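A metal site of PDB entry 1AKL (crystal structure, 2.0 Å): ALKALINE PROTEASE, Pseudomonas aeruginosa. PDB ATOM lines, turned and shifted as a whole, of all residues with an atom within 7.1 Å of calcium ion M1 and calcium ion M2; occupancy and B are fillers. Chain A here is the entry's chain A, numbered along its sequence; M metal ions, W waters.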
ATOM      1  N   GLU A 329      -0.694  -4.859 -28.007  1.00  0.00           N
ATOM      2  CA  GLU A 329       0.140  -5.158 -26.871  1.00  0.00           C
ATOM      3  C   GLU A 329       0.144  -4.224 -25.678  1.00  0.00           C
ATOM      4  O   GLU A 329       0.255  -4.696 -24.557  1.00  0.00           O
ATOM      5  CB  GLU A 329       1.585  -5.366 -27.310  1.00  0.00           C
ATOM      6  CG  GLU A 329       1.838  -6.621 -28.087  1.00  0.00           C
ATOM      7  CD  GLU A 329       1.398  -6.535 -29.525  1.00  0.00           C
ATOM      8  OE1 GLU A 329       1.019  -5.447 -30.004  1.00  0.00           O
ATOM      9  OE2 GLU A 329       1.446  -7.576 -30.205  1.00  0.00           O
ATOM     10  N   ILE A 341      -6.960  -3.784 -18.414  1.00  0.00           N
ATOM     11  CA  ILE A 341      -6.812  -5.223 -18.382  1.00  0.00           C
ATOM     12  C   ILE A 341      -6.114  -5.721 -19.650  1.00  0.00           C
ATOM     13  O   ILE A 341      -6.524  -5.388 -20.755  1.00  0.00           O
ATOM     14  CB  ILE A 341      -8.169  -5.976 -18.013  1.00  0.00           C
ATOM     15  CG1 ILE A 341      -8.682  -6.841 -19.171  1.00  0.00           C
ATOM     16  CG2 ILE A 341      -9.261  -5.029 -17.512  1.00  0.00           C
ATOM     17  CD1 ILE A 341      -8.398  -8.285 -18.954  1.00  0.00           C
ATOM     18  N   GLY A 342      -5.030  -6.478 -19.474  1.00  0.00           N
ATOM     19  CA  GLY A 342      -4.274  -6.999 -20.599  1.00  0.00           C
ATOM     20  C   GLY A 342      -4.805  -8.299 -21.152  1.00  0.00           C
ATOM     21  O   GLY A 342      -5.794  -8.832 -20.692  1.00  0.00           O
ATOM     22  N   ASN A 343      -4.135  -8.798 -22.185  1.00  0.00           N
ATOM     23  CA  ASN A 343      -4.543 -10.045 -22.805  1.00  0.00           C
ATOM     24  C   ASN A 343      -3.506 -11.104 -22.516  1.00  0.00           C
ATOM     25  O   ASN A 343      -2.648 -10.901 -21.650  1.00  0.00           O
ATOM     26  CB  ASN A 343      -4.761  -9.870 -24.306  1.00  0.00           C
ATOM     27  CG  ASN A 343      -3.582  -9.221 -24.991  1.00  0.00           C
ATOM     28  OD1 ASN A 343      -2.440  -9.398 -24.576  1.00  0.00           O
ATOM     29  ND2 ASN A 343      -3.848  -8.433 -26.028  1.00  0.00           N
ATOM     30  N   ASP A 344      -3.511 -12.190 -23.264  1.00  0.00           N
ATOM     31  CA  ASP A 344      -2.586 -13.288 -23.028  1.00  0.00           C
ATOM     32  C   ASP A 344      -1.101 -13.026 -23.233  1.00  0.00           C
ATOM     33  O   ASP A 344      -0.278 -13.669 -22.580  1.00  0.00           O
ATOM     34  CB  ASP A 344      -3.034 -14.536 -23.806  1.00  0.00           C
ATOM     35  CG  ASP A 344      -4.379 -15.090 -23.313  1.00  0.00           C
ATOM     36  OD1 ASP A 344      -4.884 -14.623 -22.274  1.00  0.00           O
ATOM     37  OD2 ASP A 344      -4.954 -15.985 -23.967  1.00  0.00           O
ATOM     38  N   VAL A 345      -0.749 -12.103 -24.119  1.00  0.00           N
ATOM     39  CA  VAL A 345       0.664 -11.822 -24.364  1.00  0.00           C
ATOM     40  C   VAL A 345       1.237 -10.862 -23.340  1.00  0.00           C
ATOM     41  O   VAL A 345       0.534 -10.430 -22.408  1.00  0.00           O
ATOM     42  CB  VAL A 345       0.908 -11.298 -25.797  1.00  0.00           C
ATOM     43  CG1 VAL A 345       0.363 -12.265 -26.822  1.00  0.00           C
ATOM     44  CG2 VAL A 345       0.298  -9.924 -25.977  1.00  0.00           C
ATOM     45  N   ALA A 346       2.526 -10.574 -23.480  1.00  0.00           N
ATOM     46  CA  ALA A 346       3.226  -9.661 -22.573  1.00  0.00           C
ATOM     47  C   ALA A 346       2.789  -8.271 -22.948  1.00  0.00           C
ATOM     48  O   ALA A 346       2.879  -7.888 -24.099  1.00  0.00           O
ATOM     49  CB  ALA A 346       4.721  -9.805 -22.734  1.00  0.00           C
ATOM     50  N   ASN A 347       2.349  -7.511 -21.956  1.00  0.00           N
ATOM     51  CA  ASN A 347       1.831  -6.179 -22.217  1.00  0.00           C
ATOM     52  C   ASN A 347       2.527  -5.142 -21.394  1.00  0.00           C
ATOM     53  O   ASN A 347       3.121  -5.452 -20.371  1.00  0.00           O
ATOM     54  CB  ASN A 347       0.344  -6.098 -21.817  1.00  0.00           C
ATOM     55  CG  ASN A 347      -0.496  -7.213 -22.388  1.00  0.00           C
ATOM     56  OD1 ASN A 347      -1.131  -7.984 -21.641  1.00  0.00           O
ATOM     57  ND2 ASN A 347      -0.514  -7.335 -23.703  1.00  0.00           N
ATOM     58  N   LEU A 349       1.409  -1.881 -19.547  1.00  0.00           N
ATOM     59  CA  LEU A 349       0.220  -1.164 -19.126  1.00  0.00           C
ATOM     60  C   LEU A 349       0.717  -0.023 -18.279  1.00  0.00           C
ATOM     61  O   LEU A 349       1.520  -0.231 -17.373  1.00  0.00           O
ATOM     62  CB  LEU A 349      -0.679  -2.063 -18.270  1.00  0.00           C
ATOM     63  CG  LEU A 349      -1.731  -2.987 -18.887  1.00  0.00           C
ATOM     64  CD1 LEU A 349      -1.239  -3.633 -20.143  1.00  0.00           C
ATOM     65  CD2 LEU A 349      -2.142  -4.044 -17.878  1.00  0.00           C
ATOM     66  N   TYR A 359      -4.381  -5.143 -14.463  1.00  0.00           N
ATOM     67  CA  TYR A 359      -4.515  -6.592 -14.503  1.00  0.00           C
ATOM     68  C   TYR A 359      -3.790  -6.999 -15.770  1.00  0.00           C
ATOM     69  O   TYR A 359      -4.250  -6.729 -16.867  1.00  0.00           O
ATOM     70  CB  TYR A 359      -6.005  -6.958 -14.582  1.00  0.00           C
ATOM     71  CG  TYR A 359      -6.309  -8.453 -14.539  1.00  0.00           C
ATOM     72  CD1 TYR A 359      -6.349  -9.208 -15.709  1.00  0.00           C
ATOM     73  CD2 TYR A 359      -6.558  -9.094 -13.337  1.00  0.00           C
ATOM     74  CE1 TYR A 359      -6.626 -10.556 -15.675  1.00  0.00           C
ATOM     75  CE2 TYR A 359      -6.836 -10.450 -13.292  1.00  0.00           C
ATOM     76  CZ  TYR A 359      -6.871 -11.169 -14.461  1.00  0.00           C
ATOM     77  OH  TYR A 359      -7.143 -12.512 -14.414  1.00  0.00           O
ATOM     78  N   GLY A 360      -2.626  -7.627 -15.620  1.00  0.00           N
ATOM     79  CA  GLY A 360      -1.865  -8.024 -16.794  1.00  0.00           C
ATOM     80  C   GLY A 360      -2.298  -9.276 -17.529  1.00  0.00           C
ATOM     81  O   GLY A 360      -1.963  -9.434 -18.715  1.00  0.00           O
ATOM     82  N   GLY A 361      -2.972 -10.191 -16.832  1.00  0.00           N
ATOM     83  CA  GLY A 361      -3.411 -11.438 -17.439  1.00  0.00           C
ATOM     84  C   GLY A 361      -2.212 -12.335 -17.665  1.00  0.00           C
ATOM     85  O   GLY A 361      -1.169 -12.151 -17.028  1.00  0.00           O
ATOM     86  N   LEU A 362      -2.338 -13.290 -18.579  1.00  0.00           N
ATOM     87  CA  LEU A 362      -1.241 -14.187 -18.891  1.00  0.00           C
ATOM     88  C   LEU A 362      -0.039 -13.414 -19.417  1.00  0.00           C
ATOM     89  O   LEU A 362      -0.132 -12.217 -19.722  1.00  0.00           O
ATOM     90  CB  LEU A 362      -1.663 -15.245 -19.906  1.00  0.00           C
ATOM     91  CG  LEU A 362      -2.753 -16.202 -19.431  1.00  0.00           C
ATOM     92  CD1 LEU A 362      -2.894 -17.314 -20.456  1.00  0.00           C
ATOM     93  CD2 LEU A 362      -2.409 -16.791 -18.090  1.00  0.00           C
ATOM     94  N   GLY A 363       1.101 -14.104 -19.477  1.00  0.00           N
ATOM     95  CA  GLY A 363       2.327 -13.495 -19.946  1.00  0.00           C
ATOM     96  C   GLY A 363       3.044 -12.639 -18.909  1.00  0.00           C
ATOM     97  O   GLY A 363       2.442 -12.247 -17.887  1.00  0.00           O
ATOM     98  N   ALA A 364       4.292 -12.311 -19.213  1.00  0.00           N
ATOM     99  CA  ALA A 364       5.154 -11.495 -18.365  1.00  0.00           C
ATOM    100  C   ALA A 364       4.942 -10.051 -18.722  1.00  0.00           C
ATOM    101  O   ALA A 364       5.527  -9.538 -19.671  1.00  0.00           O
ATOM    102  CB  ALA A 364       6.597 -11.872 -18.575  1.00  0.00           C
ATOM    103  N   ASP A 365       4.159  -9.353 -17.912  1.00  0.00           N
ATOM    104  CA  ASP A 365       3.850  -7.978 -18.193  1.00  0.00           C
ATOM    105  C   ASP A 365       4.733  -7.000 -17.460  1.00  0.00           C
ATOM    106  O   ASP A 365       5.328  -7.334 -16.437  1.00  0.00           O
ATOM    107  CB  ASP A 365       2.395  -7.707 -17.841  1.00  0.00           C
ATOM    108  CG  ASP A 365       1.462  -8.773 -18.326  1.00  0.00           C
ATOM    109  OD1 ASP A 365       1.252  -8.899 -19.554  1.00  0.00           O
ATOM    110  OD2 ASP A 365       0.934  -9.499 -17.485  1.00  0.00           O
ATOM    111  N   LEU A 367       4.159  -3.729 -15.664  1.00  0.00           N
ATOM    112  CA  LEU A 367       3.104  -2.884 -15.154  1.00  0.00           C
ATOM    113  C   LEU A 367       3.630  -1.623 -14.516  1.00  0.00           C
ATOM    114  O   LEU A 367       4.510  -1.681 -13.664  1.00  0.00           O
ATOM    115  CB  LEU A 367       2.278  -3.678 -14.138  1.00  0.00           C
ATOM    116  CG  LEU A 367       1.179  -4.638 -14.629  1.00  0.00           C
ATOM    117  CD1 LEU A 367       1.438  -5.161 -16.011  1.00  0.00           C
ATOM    118  CD2 LEU A 367       0.996  -5.784 -13.647  1.00  0.00           C
ATOM    119  N   TYR A 378      -4.383  -9.935  -9.621  1.00  0.00           N
ATOM    120  CA  TYR A 378      -4.054 -11.260 -10.136  1.00  0.00           C
ATOM    121  C   TYR A 378      -5.221 -12.174  -9.818  1.00  0.00           C
ATOM    122  O   TYR A 378      -5.830 -12.049  -8.757  1.00  0.00           O
ATOM    123  CB  TYR A 378      -2.776 -11.818  -9.482  1.00  0.00           C
ATOM    124  CG  TYR A 378      -1.537 -11.020  -9.833  1.00  0.00           C
ATOM    125  CD1 TYR A 378      -1.294  -9.798  -9.210  1.00  0.00           C
ATOM    126  CD2 TYR A 378      -0.692 -11.430 -10.854  1.00  0.00           C
ATOM    127  CE1 TYR A 378      -0.246  -8.995  -9.619  1.00  0.00           C
ATOM    128  CE2 TYR A 378       0.374 -10.623 -11.249  1.00  0.00           C
ATOM    129  CZ  TYR A 378       0.576  -9.402 -10.632  1.00  0.00           C
ATOM    130  OH  TYR A 378       1.575  -8.555 -11.059  1.00  0.00           O
ATOM    131  N   ALA A 382      -0.909 -18.740 -12.852  1.00  0.00           N
ATOM    132  CA  ALA A 382      -0.245 -18.813 -14.143  1.00  0.00           C
ATOM    133  C   ALA A 382      -0.048 -17.446 -14.779  1.00  0.00           C
ATOM    134  O   ALA A 382       0.667 -17.305 -15.776  1.00  0.00           O
ATOM    135  CB  ALA A 382      -1.017 -19.714 -15.096  1.00  0.00           C
ATOM    136  N   GLU A 383      -0.674 -16.421 -14.200  1.00  0.00           N
ATOM    137  CA  GLU A 383      -0.550 -15.083 -14.725  1.00  0.00           C
ATOM    138  C   GLU A 383       0.784 -14.453 -14.370  1.00  0.00           C
ATOM    139  O   GLU A 383       1.115 -13.376 -14.859  1.00  0.00           O
ATOM    140  CB  GLU A 383      -1.715 -14.215 -14.249  1.00  0.00           C
ATOM    141  CG  GLU A 383      -3.034 -14.706 -14.773  1.00  0.00           C
ATOM    142  CD  GLU A 383      -4.225 -13.964 -14.199  1.00  0.00           C
ATOM    143  OE1 GLU A 383      -4.048 -13.135 -13.274  1.00  0.00           O
ATOM    144  OE2 GLU A 383      -5.338 -14.222 -14.697  1.00  0.00           O
ATOM    145  N   SER A 384       1.550 -15.118 -13.529  1.00  0.00           N
ATOM    146  CA  SER A 384       2.853 -14.604 -13.141  1.00  0.00           C
ATOM    147  C   SER A 384       3.638 -15.809 -12.632  1.00  0.00           C
ATOM    148  O   SER A 384       3.989 -15.917 -11.453  1.00  0.00           O
ATOM    149  CB  SER A 384       2.694 -13.529 -12.068  1.00  0.00           C
ATOM    150  OG  SER A 384       3.741 -12.579 -12.118  1.00  0.00           O
ATOM    151  N   SER A 385       3.825 -16.774 -13.528  1.00  0.00           N
ATOM    152  CA  SER A 385       4.552 -17.976 -13.202  1.00  0.00           C
ATOM    153  C   SER A 385       5.932 -17.568 -12.742  1.00  0.00           C
ATOM    154  O   SER A 385       6.352 -16.434 -12.934  1.00  0.00           O
ATOM    155  CB  SER A 385       4.681 -18.848 -14.438  1.00  0.00           C
ATOM    156  OG  SER A 385       5.320 -18.143 -15.485  1.00  0.00           O
ATOM    157  N   ALA A 388       7.956 -17.107 -15.973  1.00  0.00           N
ATOM    158  CA  ALA A 388       7.779 -15.858 -16.721  1.00  0.00           C
ATOM    159  C   ALA A 388       7.005 -14.862 -15.873  1.00  0.00           C
ATOM    160  O   ALA A 388       5.837 -14.575 -16.137  1.00  0.00           O
ATOM    161  CB  ALA A 388       7.047 -16.137 -18.021  1.00  0.00           C
ATOM    162  N   PRO A 389       7.638 -14.305 -14.851  1.00  0.00           N
ATOM    163  CA  PRO A 389       6.993 -13.344 -13.949  1.00  0.00           C
ATOM    164  C   PRO A 389       6.774 -11.941 -14.489  1.00  0.00           C
ATOM    165  O   PRO A 389       7.455 -11.491 -15.402  1.00  0.00           O
ATOM    166  CB  PRO A 389       7.940 -13.331 -12.758  1.00  0.00           C
ATOM    167  CG  PRO A 389       9.274 -13.471 -13.411  1.00  0.00           C
ATOM    168  CD  PRO A 389       9.023 -14.575 -14.418  1.00  0.00           C
ATOM    169  N   ASP A 390       5.802 -11.247 -13.895  1.00  0.00           N
ATOM    170  CA  ASP A 390       5.487  -9.871 -14.229  1.00  0.00           C
ATOM    171  C   ASP A 390       6.631  -9.043 -13.636  1.00  0.00           C
ATOM    172  O   ASP A 390       7.499  -9.592 -12.968  1.00  0.00           O
ATOM    173  CB  ASP A 390       4.208  -9.412 -13.507  1.00  0.00           C
ATOM    174  CG  ASP A 390       2.924  -9.804 -14.227  1.00  0.00           C
ATOM    175  OD1 ASP A 390       2.958 -10.425 -15.296  1.00  0.00           O
ATOM    176  OD2 ASP A 390       1.854  -9.454 -13.692  1.00  0.00           O
HETATM  177 CA    CA M   1      -0.811 -10.100 -20.536  1.00  0.00          CA
HETATM  178 CA    CA M   2       1.006 -11.597 -16.214  1.00  0.00          CA
HETATM  179  O   HOH W   1      -0.356 -10.238 -14.897  1.00  0.00           O
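Calcium ion M2 is bound by O of Glu 383, O of Gly 363, water W1, O of Gly 361, OD2 of Asp 365 and OD1 of Asp 390.
Calcium ion M2 has six donor atoms within binding distance.
The side-chain carboxylate (OD2) of Asp 390 sits at hydrogen-bond distance from the side-chain hydroxyl (OH) of Tyr 378 (2.8 Å).
The side-chain carboxylate (OE2) of Glu 383 sits at hydrogen-bond distance from the side-chain hydroxyl (OH) of Tyr 359 (2.5 Å).
N of Asp 390 sits at hydrogen-bond distance from OG of Ser 384 (3.0 Å).
N of Gly 363 lies within hydrogen-bond range of O of Asp 344, 3.4 Å away.
The side-chain amide nitrogen of Asn 347 sits at hydrogen-bond distance from the backbone carbonyl oxygen of Glu 329 (2.9 Å).
The backbone NH of Val 345 lies close to the side-chain amide oxygen of Asn 343 (3.2 Å).
Water W1 bridges the side-chain carboxylate (OD2) of Asp 390 (2.6 Å) and the backbone NH (N) of Gly 361 (3.3 Å).
Calcium ion M1 is bound by the backbone carbonyl oxygen (O) of Gly 360 (2.3 Å).
O of Asn 343 binds calcium ion M1 (2.3 Å).
Calcium ion M1 is bound by O of Val 345 (2.3 Å).
Calcium ion M1 is bound by O of Leu 362 (2.4 Å).
Calcium ion M1 is bound by OD1 of Asn 347 (2.4 Å).
Calcium ion M1 is bound by OD1 of Asp 365 (2.6 Å).
Calcium ion M1 has six donor atoms within binding distance.
Of the 25 residues printed, 6 come within 4 Å of calcium ion M2.
Residues that only touch calcium ion M1: Asp 344 (3.99 Å).
Eight residues have an atom within 4 Å of calcium ion M1: Asn 343, Asp 344, Val 345, Asn 347, Gly 360, Gly 361, Leu 362 and Asp 365.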
